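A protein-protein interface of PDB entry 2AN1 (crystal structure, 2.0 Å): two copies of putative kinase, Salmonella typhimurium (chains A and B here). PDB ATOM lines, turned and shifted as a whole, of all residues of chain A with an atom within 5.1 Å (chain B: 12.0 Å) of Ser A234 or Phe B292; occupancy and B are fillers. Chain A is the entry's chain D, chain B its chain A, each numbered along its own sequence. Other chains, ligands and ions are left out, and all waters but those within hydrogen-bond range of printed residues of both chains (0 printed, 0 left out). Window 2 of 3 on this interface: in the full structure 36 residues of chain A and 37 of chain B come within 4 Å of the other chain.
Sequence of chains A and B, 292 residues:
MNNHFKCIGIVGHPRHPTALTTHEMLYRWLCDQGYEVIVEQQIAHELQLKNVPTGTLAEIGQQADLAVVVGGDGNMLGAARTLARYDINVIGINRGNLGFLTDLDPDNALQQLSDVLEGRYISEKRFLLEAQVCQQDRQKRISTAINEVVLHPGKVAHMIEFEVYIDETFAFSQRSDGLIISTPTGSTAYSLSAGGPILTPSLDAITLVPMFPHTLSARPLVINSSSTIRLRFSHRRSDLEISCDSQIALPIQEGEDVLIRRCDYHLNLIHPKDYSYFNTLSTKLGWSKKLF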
ATOM      1  N   GLU A 161      -7.317  28.092  27.319  1.00  0.00           N
ATOM      2  CA  GLU A 161      -7.120  28.269  25.875  1.00  0.00           C
ATOM      3  C   GLU A 161      -8.229  27.580  25.098  1.00  0.00           C
ATOM      4  O   GLU A 161      -8.631  26.459  25.432  1.00  0.00           O
ATOM      5  CB  GLU A 161      -5.768  27.714  25.404  1.00  0.00           C
ATOM      6  CG  GLU A 161      -4.583  28.107  26.264  1.00  0.00           C
ATOM      7  CD  GLU A 161      -3.262  27.685  25.659  1.00  0.00           C
ATOM      8  OE1 GLU A 161      -3.158  26.528  25.185  1.00  0.00           O
ATOM      9  OE2 GLU A 161      -2.320  28.509  25.661  1.00  0.00           O
ATOM     10  N   PHE A 162      -8.703  28.243  24.047  1.00  0.00           N
ATOM     11  CA  PHE A 162      -9.762  27.688  23.203  1.00  0.00           C
ATOM     12  C   PHE A 162      -9.679  28.236  21.789  1.00  0.00           C
ATOM     13  O   PHE A 162      -9.152  29.325  21.571  1.00  0.00           O
ATOM     14  CB  PHE A 162     -11.167  27.922  23.799  1.00  0.00           C
ATOM     15  CG  PHE A 162     -11.468  29.367  24.116  1.00  0.00           C
ATOM     16  CD1 PHE A 162     -12.175  30.157  23.215  1.00  0.00           C
ATOM     17  CD2 PHE A 162     -11.043  29.936  25.314  1.00  0.00           C
ATOM     18  CE1 PHE A 162     -12.454  31.497  23.504  1.00  0.00           C
ATOM     19  CE2 PHE A 162     -11.315  31.287  25.609  1.00  0.00           C
ATOM     20  CZ  PHE A 162     -12.022  32.054  24.703  1.00  0.00           C
ATOM     21  N   GLU A 163     -10.190  27.455  20.843  1.00  0.00           N
ATOM     22  CA  GLU A 163     -10.358  27.874  19.459  1.00  0.00           C
ATOM     23  C   GLU A 163     -11.828  28.148  19.208  1.00  0.00           C
ATOM     24  O   GLU A 163     -12.696  27.366  19.603  1.00  0.00           O
ATOM     25  CB  GLU A 163      -9.907  26.781  18.497  1.00  0.00           C
ATOM     26  CG  GLU A 163      -8.444  26.415  18.595  1.00  0.00           C
ATOM     27  CD  GLU A 163      -8.073  25.255  17.680  1.00  0.00           C
ATOM     28  OE1 GLU A 163      -8.976  24.542  17.164  1.00  0.00           O
ATOM     29  OE2 GLU A 163      -6.859  25.054  17.491  1.00  0.00           O
ATOM     30  N   ARG A 232     -13.439  24.676  20.676  1.00  0.00           N
ATOM     31  CA  ARG A 232     -12.572  23.503  20.805  1.00  0.00           C
ATOM     32  C   ARG A 232     -11.438  23.803  21.768  1.00  0.00           C
ATOM     33  O   ARG A 232     -10.991  24.953  21.884  1.00  0.00           O
ATOM     34  CB  ARG A 232     -11.997  23.077  19.453  1.00  0.00           C
ATOM     35  CG  ARG A 232     -13.029  22.566  18.472  1.00  0.00           C
ATOM     36  CD  ARG A 232     -12.347  21.807  17.344  1.00  0.00           C
ATOM     37  NE  ARG A 232     -13.273  21.505  16.253  1.00  0.00           N
ATOM     38  CZ  ARG A 232     -14.012  20.407  16.175  1.00  0.00           C
ATOM     39  NH1 ARG A 232     -13.945  19.480  17.127  1.00  0.00           N
ATOM     40  NH2 ARG A 232     -14.822  20.237  15.135  1.00  0.00           N
ATOM     41  N   PHE A 233     -10.959  22.747  22.418  1.00  0.00           N
ATOM     42  CA  PHE A 233     -10.069  22.834  23.571  1.00  0.00           C
ATOM     43  C   PHE A 233      -8.872  21.883  23.420  1.00  0.00           C
ATOM     44  O   PHE A 233      -8.884  20.990  22.570  1.00  0.00           O
ATOM     45  CB  PHE A 233     -10.880  22.522  24.834  1.00  0.00           C
ATOM     46  CG  PHE A 233     -12.192  23.270  24.906  1.00  0.00           C
ATOM     47  CD1 PHE A 233     -12.210  24.655  25.088  1.00  0.00           C
ATOM     48  CD2 PHE A 233     -13.407  22.595  24.789  1.00  0.00           C
ATOM     49  CE1 PHE A 233     -13.416  25.355  25.144  1.00  0.00           C
ATOM     50  CE2 PHE A 233     -14.625  23.282  24.851  1.00  0.00           C
ATOM     51  CZ  PHE A 233     -14.633  24.673  25.024  1.00  0.00           C
ATOM     52  N   SER A 234      -7.827  22.087  24.222  1.00  0.00           N
ATOM     53  CA  SER A 234      -6.653  21.225  24.137  1.00  0.00           C
ATOM     54  C   SER A 234      -7.041  19.820  24.549  1.00  0.00           C
ATOM     55  O   SER A 234      -7.990  19.630  25.315  1.00  0.00           O
ATOM     56  CB  SER A 234      -5.490  21.740  24.991  1.00  0.00           C
ATOM     57  OG  SER A 234      -5.679  21.452  26.362  1.00  0.00           O
ATOM     58  N   HIS A 235      -6.312  18.842  24.026  1.00  0.00           N
ATOM     59  CA  HIS A 235      -6.619  17.441  24.283  1.00  0.00           C
ATOM     60  C   HIS A 235      -6.094  17.000  25.645  1.00  0.00           C
ATOM     61  O   HIS A 235      -6.480  15.949  26.159  1.00  0.00           O
ATOM     62  CB  HIS A 235      -6.044  16.556  23.165  1.00  0.00           C
ATOM     63  CG  HIS A 235      -6.411  17.015  21.785  1.00  0.00           C
ATOM     64  ND1 HIS A 235      -7.659  16.795  21.232  1.00  0.00           N
ATOM     65  CD2 HIS A 235      -5.700  17.694  20.852  1.00  0.00           C
ATOM     66  CE1 HIS A 235      -7.696  17.317  20.016  1.00  0.00           C
ATOM     67  NE2 HIS A 235      -6.520  17.867  19.761  1.00  0.00           N
ATOM     68  N   ARG A 236      -5.230  17.822  26.231  1.00  0.00           N
ATOM     69  CA  ARG A 236      -4.500  17.455  27.437  1.00  0.00           C
ATOM     70  C   ARG A 236      -4.946  18.282  28.633  1.00  0.00           C
ATOM     71  O   ARG A 236      -5.867  17.886  29.344  1.00  0.00           O
ATOM     72  CB  ARG A 236      -2.983  17.592  27.212  1.00  0.00           C
ATOM     73  CG  ARG A 236      -2.475  17.144  25.818  1.00  0.00           C
ATOM     74  CD  ARG A 236      -2.705  15.643  25.537  1.00  0.00           C
ATOM     75  NE  ARG A 236      -2.125  15.215  24.259  1.00  0.00           N
ATOM     76  CZ  ARG A 236      -1.974  13.945  23.876  1.00  0.00           C
ATOM     77  NH1 ARG A 236      -2.364  12.949  24.666  1.00  0.00           N
ATOM     78  NH2 ARG A 236      -1.426  13.662  22.697  1.00  0.00           N
ATOM     79  N   SER B 288      -4.658  35.507  17.872  1.00  0.00           N
ATOM     80  CA  SER B 288      -3.996  34.192  17.755  1.00  0.00           C
ATOM     81  C   SER B 288      -4.702  33.257  16.777  1.00  0.00           C
ATOM     82  O   SER B 288      -5.927  33.303  16.627  1.00  0.00           O
ATOM     83  CB  SER B 288      -3.888  33.511  19.114  1.00  0.00           C
ATOM     84  OG  SER B 288      -3.456  34.424  20.098  1.00  0.00           O
ATOM     85  N   LYS B 289      -3.911  32.410  16.132  1.00  0.00           N
ATOM     86  CA  LYS B 289      -4.397  31.437  15.156  1.00  0.00           C
ATOM     87  C   LYS B 289      -4.537  30.065  15.824  1.00  0.00           C
ATOM     88  O   LYS B 289      -4.623  29.995  17.048  1.00  0.00           O
ATOM     89  CB  LYS B 289      -3.437  31.368  13.962  1.00  0.00           C
ATOM     90  CG  LYS B 289      -3.146  32.722  13.316  1.00  0.00           C
ATOM     91  CD  LYS B 289      -4.281  33.189  12.417  1.00  0.00           C
ATOM     92  CE  LYS B 289      -4.179  34.679  12.112  1.00  0.00           C
ATOM     93  NZ  LYS B 289      -3.090  35.013  11.160  1.00  0.00           N
ATOM     94  N   LYS B 290      -4.584  28.986  15.039  1.00  0.00           N
ATOM     95  CA  LYS B 290      -4.815  27.642  15.604  1.00  0.00           C
ATOM     96  C   LYS B 290      -3.802  27.289  16.686  1.00  0.00           C
ATOM     97  O   LYS B 290      -2.633  27.663  16.606  1.00  0.00           O
ATOM     98  CB  LYS B 290      -4.822  26.553  14.524  1.00  0.00           C
ATOM     99  CG  LYS B 290      -6.126  26.453  13.748  1.00  0.00           C
ATOM    100  CD  LYS B 290      -5.974  25.525  12.550  1.00  0.00           C
ATOM    101  CE  LYS B 290      -7.146  25.669  11.576  1.00  0.00           C
ATOM    102  NZ  LYS B 290      -8.289  24.783  11.952  1.00  0.00           N
ATOM    103  N   LEU B 291      -4.273  26.586  17.708  1.00  0.00           N
ATOM    104  CA  LEU B 291      -3.416  26.187  18.809  1.00  0.00           C
ATOM    105  C   LEU B 291      -3.145  24.688  18.813  1.00  0.00           C
ATOM    106  O   LEU B 291      -2.002  24.259  19.014  1.00  0.00           O
ATOM    107  CB  LEU B 291      -4.032  26.615  20.149  1.00  0.00           C
ATOM    108  CG  LEU B 291      -4.157  28.114  20.407  1.00  0.00           C
ATOM    109  CD1 LEU B 291      -4.701  28.380  21.805  1.00  0.00           C
ATOM    110  CD2 LEU B 291      -2.829  28.844  20.185  1.00  0.00           C
ATOM    111  N   PHE B 292      -4.195  23.907  18.573  1.00  0.00           N
ATOM    112  CA  PHE B 292      -4.178  22.475  18.854  1.00  0.00           C
ATOM    113  C   PHE B 292      -3.947  21.630  17.603  1.00  0.00           C
ATOM    114  O   PHE B 292      -3.211  20.641  17.645  1.00  0.00           O
ATOM    115  CB  PHE B 292      -5.469  22.061  19.573  1.00  0.00           C
ATOM    116  CG  PHE B 292      -5.912  23.029  20.636  1.00  0.00           C
ATOM    117  CD1 PHE B 292      -5.075  23.347  21.709  1.00  0.00           C
ATOM    118  CD2 PHE B 292      -7.173  23.619  20.573  1.00  0.00           C
ATOM    119  CE1 PHE B 292      -5.483  24.247  22.692  1.00  0.00           C
ATOM    120  CE2 PHE B 292      -7.591  24.514  21.550  1.00  0.00           C
ATOM    121  CZ  PHE B 292      -6.749  24.828  22.616  1.00  0.00           C
ATOM    122  OXT PHE B 292      -4.471  21.913  16.524  1.00  0.00           O
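N of Phe B292 lies within hydrogen-bond range of OE2 of Glu A163 (3.1 Å). The backbone NH of Leu B291 is in hydrogen-bond range of the side-chain carboxylate of Glu A163.
O of Arg A232 sits at hydrogen-bond distance from N of Glu A163.
Among the printed residues, pairs that only touch across the chains: Glu A161 with Leu B291, Glu A161 with Phe B292, Glu A163 with Lys B290, Arg A232 with Phe B292, Phe A233 with Phe B292 and Ser A234 with Phe B292.
Ser A234 touches just one residue of chain B: Phe B292 (3.4 Å). Of the printed residues of chain A, Phe B292 touches Glu A161, Glu A163, Arg A232, Phe A233 and Ser A234. Glu A161 touches just these residues of chain B: Leu B291 and Phe B292. Of chain B, only Phe B292 comes within 4 Å of Phe A233. No residue of chain B comes within 4 Å of His A235. Of the printed residues of chain B, Arg A232 touches Phe B292 (3.4 Å). Of the printed residues of chain A, Lys B290 touches Glu A163. Of the printed residues of chain A, Leu B291 touches Glu A161 and Glu A163. Lys B289 touches none of the printed residues of chain A. Arg A236 touches none of the printed residues of chain B.
Of the 8 printed residues of chain A, 5 touch a printed residue of chain B. Among the printed residues, 8 pairs touch across the chains. Among the printed residues, no Asp or Glu carboxylate lies within 4 Å of a Lys or Arg side-chain nitrogen of the other chain.
No position is printed for both chains.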
